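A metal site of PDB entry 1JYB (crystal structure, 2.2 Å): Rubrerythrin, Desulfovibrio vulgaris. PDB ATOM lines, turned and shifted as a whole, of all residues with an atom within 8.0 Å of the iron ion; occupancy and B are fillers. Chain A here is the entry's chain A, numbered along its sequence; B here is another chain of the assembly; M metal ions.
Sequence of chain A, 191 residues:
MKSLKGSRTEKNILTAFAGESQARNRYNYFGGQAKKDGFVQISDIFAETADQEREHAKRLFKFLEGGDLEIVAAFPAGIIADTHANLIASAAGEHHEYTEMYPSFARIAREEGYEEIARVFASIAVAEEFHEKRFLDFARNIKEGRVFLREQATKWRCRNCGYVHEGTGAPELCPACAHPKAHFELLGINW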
ATOM      1  N   ARG A 157       3.951 -22.952  -0.954  1.00  0.00           N
ATOM      2  CA  ARG A 157       3.806 -21.523  -0.710  1.00  0.00           C
ATOM      3  C   ARG A 157       3.666 -20.754  -2.029  1.00  0.00           C
ATOM      4  O   ARG A 157       4.408 -21.011  -2.975  1.00  0.00           O
ATOM      5  CB  ARG A 157       5.000 -20.964   0.015  1.00  0.00           C
ATOM      6  CG  ARG A 157       4.688 -19.623   0.621  1.00  0.00           C
ATOM      7  CD  ARG A 157       5.859 -18.999   1.299  1.00  0.00           C
ATOM      8  NE  ARG A 157       6.885 -18.809   0.277  1.00  0.00           N
ATOM      9  CZ  ARG A 157       7.538 -17.653   0.116  1.00  0.00           C
ATOM     10  NH1 ARG A 157       7.293 -16.611   0.878  1.00  0.00           N
ATOM     11  NH2 ARG A 157       8.402 -17.487  -0.880  1.00  0.00           N
ATOM     12  N   CYS A 158       2.712 -19.841  -2.091  1.00  0.00           N
ATOM     13  CA  CYS A 158       2.522 -18.887  -3.159  1.00  0.00           C
ATOM     14  C   CYS A 158       3.562 -17.829  -2.945  1.00  0.00           C
ATOM     15  O   CYS A 158       3.522 -17.121  -1.931  1.00  0.00           O
ATOM     16  CB  CYS A 158       1.207 -18.224  -3.075  1.00  0.00           C
ATOM     17  SG  CYS A 158       0.814 -17.005  -4.356  1.00  0.00           S
ATOM     18  N   ARG A 159       4.427 -17.705  -3.934  1.00  0.00           N
ATOM     19  CA  ARG A 159       5.449 -16.703  -3.900  1.00  0.00           C
ATOM     20  C   ARG A 159       4.865 -15.324  -4.091  1.00  0.00           C
ATOM     21  O   ARG A 159       5.474 -14.319  -3.683  1.00  0.00           O
ATOM     22  CB  ARG A 159       6.457 -16.920  -4.972  1.00  0.00           C
ATOM     23  CG  ARG A 159       7.132 -18.253  -4.825  1.00  0.00           C
ATOM     24  CD  ARG A 159       8.093 -18.469  -5.974  1.00  0.00           C
ATOM     25  NE  ARG A 159       9.405 -18.048  -5.520  1.00  0.00           N
ATOM     26  CZ  ARG A 159       9.908 -16.868  -5.836  1.00  0.00           C
ATOM     27  NH1 ARG A 159       9.214 -16.008  -6.597  1.00  0.00           N
ATOM     28  NH2 ARG A 159      11.095 -16.514  -5.371  1.00  0.00           N
ATOM     29  N   ASN A 160       3.696 -15.220  -4.722  1.00  0.00           N
ATOM     30  CA  ASN A 160       3.130 -13.926  -4.880  1.00  0.00           C
ATOM     31  C   ASN A 160       2.494 -13.431  -3.580  1.00  0.00           C
ATOM     32  O   ASN A 160       2.799 -12.301  -3.200  1.00  0.00           O
ATOM     33  CB  ASN A 160       2.123 -13.976  -5.957  1.00  0.00           C
ATOM     34  CG  ASN A 160       1.734 -12.576  -6.405  1.00  0.00           C
ATOM     35  OD1 ASN A 160       0.548 -12.223  -6.471  1.00  0.00           O
ATOM     36  ND2 ASN A 160       2.651 -11.739  -6.864  1.00  0.00           N
ATOM     37  N   CYS A 161       1.714 -14.179  -2.787  1.00  0.00           N
ATOM     38  CA  CYS A 161       1.119 -13.561  -1.617  1.00  0.00           C
ATOM     39  C   CYS A 161       1.441 -14.261  -0.308  1.00  0.00           C
ATOM     40  O   CYS A 161       1.015 -13.788   0.760  1.00  0.00           O
ATOM     41  CB  CYS A 161      -0.381 -13.494  -1.765  1.00  0.00           C
ATOM     42  SG  CYS A 161      -1.117 -15.159  -1.666  1.00  0.00           S
ATOM     43  N   GLY A 162       2.162 -15.387  -0.347  1.00  0.00           N
ATOM     44  CA  GLY A 162       2.597 -16.112   0.830  1.00  0.00           C
ATOM     45  C   GLY A 162       1.589 -17.077   1.411  1.00  0.00           C
ATOM     46  O   GLY A 162       1.796 -17.591   2.527  1.00  0.00           O
ATOM     47  N   TYR A 163       0.500 -17.339   0.698  1.00  0.00           N
ATOM     48  CA  TYR A 163      -0.480 -18.290   1.119  1.00  0.00           C
ATOM     49  C   TYR A 163       0.150 -19.684   1.240  1.00  0.00           C
ATOM     50  O   TYR A 163       0.898 -20.095   0.347  1.00  0.00           O
ATOM     51  CB  TYR A 163      -1.628 -18.268   0.096  1.00  0.00           C
ATOM     52  CG  TYR A 163      -2.710 -19.309   0.364  1.00  0.00           C
ATOM     53  CD1 TYR A 163      -3.607 -19.143   1.400  1.00  0.00           C
ATOM     54  CD2 TYR A 163      -2.715 -20.474  -0.380  1.00  0.00           C
ATOM     55  CE1 TYR A 163      -4.558 -20.131   1.673  1.00  0.00           C
ATOM     56  CE2 TYR A 163      -3.643 -21.473  -0.107  1.00  0.00           C
ATOM     57  CZ  TYR A 163      -4.548 -21.296   0.929  1.00  0.00           C
ATOM     58  OH  TYR A 163      -5.491 -22.257   1.147  1.00  0.00           O
ATOM     59  N   VAL A 164      -0.072 -20.404   2.358  1.00  0.00           N
ATOM     60  CA  VAL A 164       0.456 -21.755   2.480  1.00  0.00           C
ATOM     61  C   VAL A 164      -0.679 -22.759   2.285  1.00  0.00           C
ATOM     62  O   VAL A 164      -1.786 -22.623   2.810  1.00  0.00           O
ATOM     63  CB  VAL A 164       1.136 -21.927   3.853  1.00  0.00           C
ATOM     64  CG1 VAL A 164       1.633 -23.379   4.020  1.00  0.00           C
ATOM     65  CG2 VAL A 164       2.305 -20.943   3.948  1.00  0.00           C
ATOM     66  N   LEU A 173      -5.245 -22.082  -8.713  1.00  0.00           N
ATOM     67  CA  LEU A 173      -5.217 -20.653  -8.521  1.00  0.00           C
ATOM     68  C   LEU A 173      -5.028 -20.468  -7.060  1.00  0.00           C
ATOM     69  O   LEU A 173      -5.666 -21.187  -6.305  1.00  0.00           O
ATOM     70  CB  LEU A 173      -6.514 -19.995  -8.855  1.00  0.00           C
ATOM     71  CG  LEU A 173      -6.869 -19.867 -10.301  1.00  0.00           C
ATOM     72  CD1 LEU A 173      -8.206 -19.197 -10.386  1.00  0.00           C
ATOM     73  CD2 LEU A 173      -5.862 -19.025 -11.041  1.00  0.00           C
ATOM     74  N   CYS A 174      -4.194 -19.580  -6.627  1.00  0.00           N
ATOM     75  CA  CYS A 174      -4.092 -19.301  -5.240  1.00  0.00           C
ATOM     76  C   CYS A 174      -5.416 -18.708  -4.687  1.00  0.00           C
ATOM     77  O   CYS A 174      -5.929 -17.713  -5.218  1.00  0.00           O
ATOM     78  CB  CYS A 174      -2.966 -18.350  -5.098  1.00  0.00           C
ATOM     79  SG  CYS A 174      -2.780 -17.743  -3.418  1.00  0.00           S
ATOM     80  N   PRO A 175      -6.052 -19.205  -3.619  1.00  0.00           N
ATOM     81  CA  PRO A 175      -7.278 -18.587  -3.089  1.00  0.00           C
ATOM     82  C   PRO A 175      -7.168 -17.189  -2.467  1.00  0.00           C
ATOM     83  O   PRO A 175      -8.182 -16.502  -2.334  1.00  0.00           O
ATOM     84  CB  PRO A 175      -7.751 -19.653  -2.144  1.00  0.00           C
ATOM     85  CG  PRO A 175      -6.502 -20.329  -1.657  1.00  0.00           C
ATOM     86  CD  PRO A 175      -5.683 -20.436  -2.910  1.00  0.00           C
ATOM     87  N   ALA A 176      -5.976 -16.770  -2.030  1.00  0.00           N
ATOM     88  CA  ALA A 176      -5.795 -15.468  -1.438  1.00  0.00           C
ATOM     89  C   ALA A 176      -5.542 -14.441  -2.523  1.00  0.00           C
ATOM     90  O   ALA A 176      -6.235 -13.422  -2.512  1.00  0.00           O
ATOM     91  CB  ALA A 176      -4.602 -15.470  -0.505  1.00  0.00           C
ATOM     92  N   CYS A 177      -4.618 -14.619  -3.501  1.00  0.00           N
ATOM     93  CA  CYS A 177      -4.284 -13.581  -4.489  1.00  0.00           C
ATOM     94  C   CYS A 177      -4.810 -13.902  -5.867  1.00  0.00           C
ATOM     95  O   CYS A 177      -4.658 -13.091  -6.781  1.00  0.00           O
ATOM     96  CB  CYS A 177      -2.759 -13.343  -4.656  1.00  0.00           C
ATOM     97  SG  CYS A 177      -1.850 -14.757  -5.381  1.00  0.00           S
ATOM     98  N   ALA A 178      -5.418 -15.076  -6.065  1.00  0.00           N
ATOM     99  CA  ALA A 178      -5.939 -15.571  -7.345  1.00  0.00           C
ATOM    100  C   ALA A 178      -4.917 -15.613  -8.473  1.00  0.00           C
ATOM    101  O   ALA A 178      -5.259 -15.421  -9.645  1.00  0.00           O
ATOM    102  CB  ALA A 178      -7.125 -14.743  -7.831  1.00  0.00           C
ATOM    103  N   HIS A 179      -3.629 -15.805  -8.190  1.00  0.00           N
ATOM    104  CA  HIS A 179      -2.639 -15.959  -9.249  1.00  0.00           C
ATOM    105  C   HIS A 179      -2.513 -17.452  -9.483  1.00  0.00           C
ATOM    106  O   HIS A 179      -2.868 -18.265  -8.623  1.00  0.00           O
ATOM    107  CB  HIS A 179      -1.296 -15.329  -8.813  1.00  0.00           C
ATOM    108  CG  HIS A 179      -1.288 -13.805  -8.920  1.00  0.00           C
ATOM    109  ND1 HIS A 179      -2.178 -12.935  -8.449  1.00  0.00           N
ATOM    110  CD2 HIS A 179      -0.328 -13.077  -9.574  1.00  0.00           C
ATOM    111  CE1 HIS A 179      -1.824 -11.723  -8.802  1.00  0.00           C
ATOM    112  NE2 HIS A 179      -0.698 -11.826  -9.474  1.00  0.00           N
ATOM    113  N   PRO A 180      -2.118 -17.912 -10.667  1.00  0.00           N
ATOM    114  CA  PRO A 180      -2.148 -19.342 -10.964  1.00  0.00           C
ATOM    115  C   PRO A 180      -1.012 -20.145 -10.349  1.00  0.00           C
ATOM    116  O   PRO A 180      -0.029 -19.608  -9.814  1.00  0.00           O
ATOM    117  CB  PRO A 180      -2.172 -19.396 -12.487  1.00  0.00           C
ATOM    118  CG  PRO A 180      -1.458 -18.140 -12.862  1.00  0.00           C
ATOM    119  CD  PRO A 180      -2.085 -17.146 -11.898  1.00  0.00           C
ATOM    120  N   HIS A 183       2.896 -19.754  -9.575  1.00  0.00           N
ATOM    121  CA  HIS A 183       3.466 -19.019  -8.442  1.00  0.00           C
ATOM    122  C   HIS A 183       3.927 -19.741  -7.199  1.00  0.00           C
ATOM    123  O   HIS A 183       4.639 -19.151  -6.373  1.00  0.00           O
ATOM    124  CB  HIS A 183       2.512 -17.987  -7.986  1.00  0.00           C
ATOM    125  CG  HIS A 183       2.563 -16.919  -9.027  1.00  0.00           C
ATOM    126  ND1 HIS A 183       3.341 -15.840  -9.007  1.00  0.00           N
ATOM    127  CD2 HIS A 183       1.849 -16.931 -10.194  1.00  0.00           C
ATOM    128  CE1 HIS A 183       3.141 -15.186 -10.119  1.00  0.00           C
ATOM    129  NE2 HIS A 183       2.228 -15.832 -10.831  1.00  0.00           N
ATOM    130  N   PHE A 184       3.552 -21.004  -7.120  1.00  0.00           N
ATOM    131  CA  PHE A 184       3.811 -21.850  -5.985  1.00  0.00           C
ATOM    132  C   PHE A 184       5.181 -22.541  -6.000  1.00  0.00           C
ATOM    133  O   PHE A 184       5.771 -22.919  -7.029  1.00  0.00           O
ATOM    134  CB  PHE A 184       2.658 -22.852  -5.930  1.00  0.00           C
ATOM    135  CG  PHE A 184       1.383 -22.346  -5.268  1.00  0.00           C
ATOM    136  CD1 PHE A 184       0.371 -21.782  -6.008  1.00  0.00           C
ATOM    137  CD2 PHE A 184       1.268 -22.389  -3.871  1.00  0.00           C
ATOM    138  CE1 PHE A 184      -0.741 -21.268  -5.362  1.00  0.00           C
ATOM    139  CE2 PHE A 184       0.149 -21.872  -3.220  1.00  0.00           C
ATOM    140  CZ  PHE A 184      -0.849 -21.306  -3.976  1.00  0.00           C
ATOM    141  N   GLN B  52       4.364  -8.906  -0.512  1.00  0.00           N
ATOM    142  CA  GLN B  52       3.224  -9.784  -0.421  1.00  0.00           C
ATOM    143  C   GLN B  52       2.079  -8.970   0.128  1.00  0.00           C
ATOM    144  O   GLN B  52       0.955  -9.201  -0.305  1.00  0.00           O
ATOM    145  CB  GLN B  52       3.581 -10.953   0.481  1.00  0.00           C
ATOM    146  CG  GLN B  52       4.604 -11.784  -0.335  1.00  0.00           C
ATOM    147  CD  GLN B  52       5.071 -13.022   0.417  1.00  0.00           C
ATOM    148  OE1 GLN B  52       5.060 -13.027   1.654  1.00  0.00           O
ATOM    149  NE2 GLN B  52       5.434 -14.096  -0.245  1.00  0.00           N
ATOM    150  N   GLU B  55       0.202  -7.377  -2.552  1.00  0.00           N
ATOM    151  CA  GLU B  55      -0.721  -8.234  -3.252  1.00  0.00           C
ATOM    152  C   GLU B  55      -1.999  -8.606  -2.561  1.00  0.00           C
ATOM    153  O   GLU B  55      -3.038  -8.834  -3.176  1.00  0.00           O
ATOM    154  CB  GLU B  55       0.023  -9.485  -3.658  1.00  0.00           C
ATOM    155  CG  GLU B  55       1.112  -9.143  -4.679  1.00  0.00           C
ATOM    156  CD  GLU B  55       0.690  -8.515  -6.029  1.00  0.00           C
ATOM    157  OE1 GLU B  55      -0.194  -9.071  -6.684  1.00  0.00           O
ATOM    158  OE2 GLU B  55       1.263  -7.502  -6.441  1.00  0.00           O
ATOM    159  N   HIS B  56      -1.966  -8.680  -1.266  1.00  0.00           N
ATOM    160  CA  HIS B  56      -3.184  -8.906  -0.522  1.00  0.00           C
ATOM    161  C   HIS B  56      -4.034  -7.630  -0.658  1.00  0.00           C
ATOM    162  O   HIS B  56      -5.243  -7.683  -0.831  1.00  0.00           O
ATOM    163  CB  HIS B  56      -2.883  -9.107   0.961  1.00  0.00           C
ATOM    164  CG  HIS B  56      -2.115 -10.370   1.328  1.00  0.00           C
ATOM    165  ND1 HIS B  56      -1.315 -10.523   2.381  1.00  0.00           N
ATOM    166  CD2 HIS B  56      -2.113 -11.561   0.639  1.00  0.00           C
ATOM    167  CE1 HIS B  56      -0.838 -11.743   2.370  1.00  0.00           C
ATOM    168  NE2 HIS B  56      -1.334 -12.350   1.317  1.00  0.00           N
ATOM    169  N   SER B 123      -8.467 -16.765   3.455  1.00  0.00           N
ATOM    170  CA  SER B 123      -7.232 -17.208   2.827  1.00  0.00           C
ATOM    171  C   SER B 123      -6.045 -16.292   3.067  1.00  0.00           C
ATOM    172  O   SER B 123      -4.922 -16.763   3.251  1.00  0.00           O
ATOM    173  CB  SER B 123      -7.459 -17.348   1.345  1.00  0.00           C
ATOM    174  OG  SER B 123      -8.353 -18.418   1.083  1.00  0.00           O
ATOM    175  N   ALA B 127      -1.676 -16.795   5.124  1.00  0.00           N
ATOM    176  CA  ALA B 127      -0.444 -16.108   4.772  1.00  0.00           C
ATOM    177  C   ALA B 127       0.013 -15.245   5.914  1.00  0.00           C
ATOM    178  O   ALA B 127       1.206 -15.108   6.176  1.00  0.00           O
ATOM    179  CB  ALA B 127      -0.701 -15.228   3.553  1.00  0.00           C
HETATM  180 FE    FE M   1      -1.174 -16.153  -3.696  1.00  0.00          FE
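Within 4 Å of the iron ion: Cys 158, Cys 161, Cys 174 and Cys 177.
Along chain A the residues within 4 Å of the iron ion span positions 158 to 177.
The nearest printed residue that does not touch the iron ion is Tyr 163 (4.4 Å).
N of Cys 174 sits at hydrogen-bond distance from O of His 179, at 2.7 Å.
The backbone carbonyl oxygen of Tyr 163 is in hydrogen-bond range of the backbone NH of Cys 158.
The backbone NH (N) of Tyr 163 lies close to the side-chain sulfur (SG) of Cys 161 (3.6 Å).
The side-chain sulfur (SG) of Cys 174 sits close to the backbone NH (N) of Ala 176 (3.6 Å).
The backbone carbonyl oxygen of Cys 177 sits at hydrogen-bond distance from a ring nitrogen (ND1) of His 179 (3.0 Å).
SG of Cys 158 lies close to N of Asn 160, at 3.4 Å.
The side-chain sulfur (SG) of Cys 177 sits close to the side-chain amide oxygen (OD1) of Asn 160, at 3.7 Å.
NE2 of His 56 of chain B lies within hydrogen-bond range of O of Cys 161 (2.8 Å).
The iron ion is bound by the side-chain sulfur of Cys 161, the side-chain sulfur of Cys 158, the side-chain sulfur of Cys 174 and the side-chain sulfur of Cys 177.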
